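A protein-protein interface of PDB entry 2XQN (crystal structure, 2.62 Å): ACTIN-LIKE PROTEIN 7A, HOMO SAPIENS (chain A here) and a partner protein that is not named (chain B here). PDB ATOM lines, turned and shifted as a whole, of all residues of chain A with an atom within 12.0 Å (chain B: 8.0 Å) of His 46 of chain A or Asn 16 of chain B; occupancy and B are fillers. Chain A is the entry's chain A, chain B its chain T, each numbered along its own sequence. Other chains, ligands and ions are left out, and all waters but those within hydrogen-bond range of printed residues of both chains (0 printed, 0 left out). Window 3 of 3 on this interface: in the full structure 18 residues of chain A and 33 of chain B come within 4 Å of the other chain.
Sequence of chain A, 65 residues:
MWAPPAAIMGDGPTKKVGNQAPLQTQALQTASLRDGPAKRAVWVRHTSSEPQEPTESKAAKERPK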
ATOM      1  N   VAL A  42      -6.844  18.309  -6.385  1.00  0.00           N
ATOM      2  CA  VAL A  42      -6.348  17.122  -5.718  1.00  0.00           C
ATOM      3  C   VAL A  42      -6.149  17.427  -4.241  1.00  0.00           C
ATOM      4  O   VAL A  42      -5.477  18.423  -3.864  1.00  0.00           O
ATOM      5  CB  VAL A  42      -5.054  16.587  -6.343  1.00  0.00           C
ATOM      6  CG1 VAL A  42      -4.501  15.407  -5.533  1.00  0.00           C
ATOM      7  CG2 VAL A  42      -5.281  16.191  -7.792  1.00  0.00           C
ATOM      8  N   TRP A  43      -6.762  16.578  -3.409  1.00  0.00           N
ATOM      9  CA  TRP A  43      -6.590  16.667  -1.964  1.00  0.00           C
ATOM     10  C   TRP A  43      -5.355  15.881  -1.577  1.00  0.00           C
ATOM     11  O   TRP A  43      -5.397  14.661  -1.537  1.00  0.00           O
ATOM     12  CB  TRP A  43      -7.795  16.101  -1.232  1.00  0.00           C
ATOM     13  CG  TRP A  43      -7.862  16.477   0.253  1.00  0.00           C
ATOM     14  CD1 TRP A  43      -6.818  16.836   1.069  1.00  0.00           C
ATOM     15  CD2 TRP A  43      -9.038  16.500   1.080  1.00  0.00           C
ATOM     16  NE1 TRP A  43      -7.268  17.093   2.336  1.00  0.00           N
ATOM     17  CE2 TRP A  43      -8.627  16.899   2.376  1.00  0.00           C
ATOM     18  CE3 TRP A  43     -10.409  16.249   0.849  1.00  0.00           C
ATOM     19  CZ2 TRP A  43      -9.549  17.050   3.450  1.00  0.00           C
ATOM     20  CZ3 TRP A  43     -11.325  16.392   1.928  1.00  0.00           C
ATOM     21  CH2 TRP A  43     -10.881  16.790   3.202  1.00  0.00           C
ATOM     22  N   VAL A  44      -4.254  16.590  -1.329  1.00  0.00           N
ATOM     23  CA  VAL A  44      -3.036  15.935  -0.910  1.00  0.00           C
ATOM     24  C   VAL A  44      -3.113  15.737   0.583  1.00  0.00           C
ATOM     25  O   VAL A  44      -3.258  16.717   1.341  1.00  0.00           O
ATOM     26  CB  VAL A  44      -1.766  16.706  -1.289  1.00  0.00           C
ATOM     27  CG1 VAL A  44      -0.526  16.031  -0.648  1.00  0.00           C
ATOM     28  CG2 VAL A  44      -1.640  16.763  -2.810  1.00  0.00           C
ATOM     29  N   ARG A  45      -3.046  14.461   0.974  1.00  0.00           N
ATOM     30  CA  ARG A  45      -3.203  14.011   2.359  1.00  0.00           C
ATOM     31  C   ARG A  45      -2.754  12.563   2.484  1.00  0.00           C
ATOM     32  O   ARG A  45      -3.092  11.724   1.643  1.00  0.00           O
ATOM     33  CB  ARG A  45      -4.656  14.138   2.817  1.00  0.00           C
ATOM     34  CG  ARG A  45      -5.588  13.062   2.286  1.00  0.00           C
ATOM     35  CD  ARG A  45      -6.968  13.323   2.722  1.00  0.00           C
ATOM     36  NE  ARG A  45      -7.858  13.218   1.577  1.00  0.00           N
ATOM     37  CZ  ARG A  45      -9.167  13.490   1.591  1.00  0.00           C
ATOM     38  NH1 ARG A  45      -9.797  13.892   2.698  1.00  0.00           N
ATOM     39  NH2 ARG A  45      -9.853  13.359   0.469  1.00  0.00           N
ATOM     40  N   HIS A  46      -1.980  12.273   3.522  1.00  0.00           N
ATOM     41  CA  HIS A  46      -1.428  10.922   3.686  1.00  0.00           C
ATOM     42  C   HIS A  46      -2.517   9.987   4.189  1.00  0.00           C
ATOM     43  O   HIS A  46      -3.572  10.437   4.639  1.00  0.00           O
ATOM     44  CB  HIS A  46      -0.200  10.904   4.614  1.00  0.00           C
ATOM     45  CG  HIS A  46       0.880  11.850   4.201  1.00  0.00           C
ATOM     46  ND1 HIS A  46       1.888  11.495   3.331  1.00  0.00           N
ATOM     47  CD2 HIS A  46       1.091  13.153   4.515  1.00  0.00           C
ATOM     48  CE1 HIS A  46       2.681  12.534   3.138  1.00  0.00           C
ATOM     49  NE2 HIS A  46       2.218  13.556   3.840  1.00  0.00           N
ATOM     50  N   THR A  47      -2.261   8.694   4.063  1.00  0.00           N
ATOM     51  CA  THR A  47      -3.106   7.633   4.560  1.00  0.00           C
ATOM     52  C   THR A  47      -2.763   7.334   6.015  1.00  0.00           C
ATOM     53  O   THR A  47      -1.576   7.338   6.385  1.00  0.00           O
ATOM     54  CB  THR A  47      -2.728   6.423   3.793  1.00  0.00           C
ATOM     55  OG1 THR A  47      -2.795   6.752   2.403  1.00  0.00           O
ATOM     56  CG2 THR A  47      -3.620   5.256   4.140  1.00  0.00           C
ATOM     57  N   SER A  48      -3.764   7.046   6.849  1.00  0.00           N
ATOM     58  CA  SER A  48      -3.458   6.718   8.256  1.00  0.00           C
ATOM     59  C   SER A  48      -2.780   5.357   8.474  1.00  0.00           C
ATOM     60  O   SER A  48      -2.789   4.487   7.578  1.00  0.00           O
ATOM     61  CB  SER A  48      -4.703   6.833   9.121  1.00  0.00           C
ATOM     62  OG  SER A  48      -4.758   8.148   9.597  1.00  0.00           O
ATOM     63  N   SER A  49      -2.173   5.190   9.651  1.00  0.00           N
ATOM     64  CA  SER A  49      -1.893   3.851  10.197  1.00  0.00           C
ATOM     65  C   SER A  49      -3.181   3.347  10.906  1.00  0.00           C
ATOM     66  O   SER A  49      -3.674   2.239  10.636  1.00  0.00           O
ATOM     67  CB  SER A  49      -0.706   3.902  11.184  1.00  0.00           C
ATOM     68  OG  SER A  49      -1.162   4.258  12.486  1.00  0.00           O
ATOM     69  N   LYS B   3       9.312  22.499   1.836  1.00  0.00           N
ATOM     70  CA  LYS B   3       7.861  22.702   2.021  1.00  0.00           C
ATOM     71  C   LYS B   3       7.251  23.369   0.749  1.00  0.00           C
ATOM     72  O   LYS B   3       7.864  24.299   0.175  1.00  0.00           O
ATOM     73  CB  LYS B   3       7.597  23.572   3.270  1.00  0.00           C
ATOM     74  CG  LYS B   3       7.864  22.876   4.625  1.00  0.00           C
ATOM     75  CD  LYS B   3       6.895  21.717   4.903  1.00  0.00           C
ATOM     76  CE  LYS B   3       7.044  21.128   6.325  1.00  0.00           C
ATOM     77  NZ  LYS B   3       8.376  20.492   6.542  1.00  0.00           N
ATOM     78  N   PRO B   4       6.062  22.899   0.299  1.00  0.00           N
ATOM     79  CA  PRO B   4       5.448  23.453  -0.909  1.00  0.00           C
ATOM     80  C   PRO B   4       4.949  24.855  -0.654  1.00  0.00           C
ATOM     81  O   PRO B   4       4.513  25.138   0.443  1.00  0.00           O
ATOM     82  CB  PRO B   4       4.285  22.514  -1.167  1.00  0.00           C
ATOM     83  CG  PRO B   4       4.007  21.898   0.154  1.00  0.00           C
ATOM     84  CD  PRO B   4       5.272  21.803   0.880  1.00  0.00           C
ATOM     85  N   ILE B  13       3.222  26.114   2.996  1.00  0.00           N
ATOM     86  CA  ILE B  13       2.228  25.293   3.633  1.00  0.00           C
ATOM     87  C   ILE B  13       2.959  24.433   4.670  1.00  0.00           C
ATOM     88  O   ILE B  13       3.867  23.686   4.310  1.00  0.00           O
ATOM     89  CB  ILE B  13       1.520  24.432   2.606  1.00  0.00           C
ATOM     90  CG1 ILE B  13       0.514  25.270   1.831  1.00  0.00           C
ATOM     91  CG2 ILE B  13       0.866  23.253   3.250  1.00  0.00           C
ATOM     92  CD1 ILE B  13       0.848  25.393   0.398  1.00  0.00           C
ATOM     93  N   PHE B  14       2.584  24.565   5.956  1.00  0.00           N
ATOM     94  CA  PHE B  14       3.171  23.723   7.029  1.00  0.00           C
ATOM     95  C   PHE B  14       2.276  22.585   7.444  1.00  0.00           C
ATOM     96  O   PHE B  14       2.759  21.583   7.929  1.00  0.00           O
ATOM     97  CB  PHE B  14       3.645  24.547   8.230  1.00  0.00           C
ATOM     98  CG  PHE B  14       4.772  25.426   7.884  1.00  0.00           C
ATOM     99  CD1 PHE B  14       6.060  24.918   7.834  1.00  0.00           C
ATOM    100  CD2 PHE B  14       4.538  26.749   7.489  1.00  0.00           C
ATOM    101  CE1 PHE B  14       7.095  25.711   7.435  1.00  0.00           C
ATOM    102  CE2 PHE B  14       5.582  27.562   7.073  1.00  0.00           C
ATOM    103  CZ  PHE B  14       6.864  27.034   7.051  1.00  0.00           C
ATOM    104  N   SER B  15       0.978  22.726   7.219  1.00  0.00           N
ATOM    105  CA  SER B  15       0.064  21.606   7.382  1.00  0.00           C
ATOM    106  C   SER B  15       0.568  20.417   6.551  1.00  0.00           C
ATOM    107  O   SER B  15       1.329  20.604   5.580  1.00  0.00           O
ATOM    108  CB  SER B  15      -1.322  22.006   6.896  1.00  0.00           C
ATOM    109  OG  SER B  15      -2.218  20.935   7.146  1.00  0.00           O
ATOM    110  N   ASN B  16       0.161  19.201   6.908  1.00  0.00           N
ATOM    111  CA  ASN B  16       0.543  18.006   6.109  1.00  0.00           C
ATOM    112  C   ASN B  16      -0.561  17.635   5.111  1.00  0.00           C
ATOM    113  O   ASN B  16      -0.535  16.558   4.498  1.00  0.00           O
ATOM    114  CB  ASN B  16       0.849  16.821   7.016  1.00  0.00           C
ATOM    115  CG  ASN B  16      -0.185  16.670   8.102  1.00  0.00           C
ATOM    116  OD1 ASN B  16      -1.090  17.510   8.251  1.00  0.00           O
ATOM    117  ND2 ASN B  16      -0.060  15.612   8.879  1.00  0.00           N
ATOM    118  N   GLU B  17      -1.531  18.544   4.977  1.00  0.00           N
ATOM    119  CA  GLU B  17      -2.600  18.446   4.001  1.00  0.00           C
ATOM    120  C   GLU B  17      -2.728  19.781   3.337  1.00  0.00           C
ATOM    121  O   GLU B  17      -2.567  20.795   3.992  1.00  0.00           O
ATOM    122  CB  GLU B  17      -3.889  18.092   4.684  1.00  0.00           C
ATOM    123  CG  GLU B  17      -3.877  16.681   5.147  1.00  0.00           C
ATOM    124  CD  GLU B  17      -5.181  16.297   5.791  1.00  0.00           C
ATOM    125  OE1 GLU B  17      -6.168  17.093   5.689  1.00  0.00           O
ATOM    126  OE2 GLU B  17      -5.202  15.185   6.386  1.00  0.00           O
ATOM    127  N   TYR B  18      -2.976  19.766   2.029  1.00  0.00           N
ATOM    128  CA  TYR B  18      -3.097  20.965   1.183  1.00  0.00           C
ATOM    129  C   TYR B  18      -3.783  20.552  -0.146  1.00  0.00           C
ATOM    130  O   TYR B  18      -4.145  19.348  -0.357  1.00  0.00           O
ATOM    131  CB  TYR B  18      -1.726  21.668   0.971  1.00  0.00           C
ATOM    132  CG  TYR B  18      -0.685  20.810   0.292  1.00  0.00           C
ATOM    133  CD1 TYR B  18       0.025  19.830   1.008  1.00  0.00           C
ATOM    134  CD2 TYR B  18      -0.417  20.957  -1.071  1.00  0.00           C
ATOM    135  CE1 TYR B  18       0.956  19.013   0.398  1.00  0.00           C
ATOM    136  CE2 TYR B  18       0.527  20.140  -1.708  1.00  0.00           C
ATOM    137  CZ  TYR B  18       1.209  19.171  -0.959  1.00  0.00           C
ATOM    138  OH  TYR B  18       2.129  18.362  -1.587  1.00  0.00           O
ATOM    139  N   LEU B  28      -5.395  24.405   2.175  1.00  0.00           N
ATOM    140  CA  LEU B  28      -6.733  23.901   1.899  1.00  0.00           C
ATOM    141  C   LEU B  28      -7.686  25.089   1.760  1.00  0.00           C
ATOM    142  O   LEU B  28      -8.493  25.141   0.818  1.00  0.00           O
ATOM    143  CB  LEU B  28      -7.240  22.980   2.996  1.00  0.00           C
ATOM    144  CG  LEU B  28      -6.694  21.569   3.224  1.00  0.00           C
ATOM    145  CD1 LEU B  28      -7.178  21.066   4.582  1.00  0.00           C
ATOM    146  CD2 LEU B  28      -7.024  20.522   2.109  1.00  0.00           C
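N of Val 44 of chain A is in hydrogen-bond range of O of Tyr 18 of chain B, 2.9 Å away.
The side-chain hydroxyl of Ser 15 of chain B sits at hydrogen-bond distance from the backbone carbonyl oxygen of Glu 17 of chain B (3.2 Å).
Of the 9 printed residues of chain B, 4 touch a printed residue of chain A. Hydrophobic or aromatic side chains of chain B within 4 Å of the printed part of chain A: Tyr 18 and Leu 28. Printed residues of chain A that touch a printed residue of chain B: Val 42, Trp 43, Val 44, Arg 45 and His 46. Among the printed residues, no Asp or Glu carboxylate lies within 4 Å of a Lys or Arg side-chain nitrogen of the other chain.
Printed residues of chain B within 4 Å of Trp 43 of chain A: Glu 17, Tyr 18 and Leu 28. Of the printed residues of chain B, Val 44 of chain A touches Glu 17 and Tyr 18. Of the printed residues of chain B, Arg 45 of chain A touches Glu 17. His 46 of chain A touches one residue of chain B. Lys 3 of chain B touches none of the printed residues of chain A. Ile 13 of chain B touches none of the printed residues of chain A. No residue of chain A comes within 4 Å of Ser 15 of chain B. Of chain A, only His 46 (3.8 Å) comes within 4 Å of Asn 16 of chain B. Glu 17 of chain B touches just these residues of chain A: Trp 43, Val 44 and Arg 45. Of the printed residues of chain A, Leu 28 of chain B touches Trp 43 (3.4 Å). The nearest residue of chain A that does not touch Asn 16 of chain B is Val 44 of chain A (4.2 Å).
O of Tyr 18 of chain B touches O of Val 42 of chain A, 3.9 Å away. Trp 43 of chain A touches Glu 17 of chain B. Tyr 18 of chain B touches Trp 43 of chain A (O to C, 3.9 Å). Trp 43 of chain A touches Leu 28 of chain B. Glu 17 of chain B touches Val 44 of chain A. CB of Arg 45 of chain A touches CG of Glu 17 of chain B (3.5 Å). CD2 of His 46 of chain A touches O of Asn 16 of chain B, 3.8 Å away.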
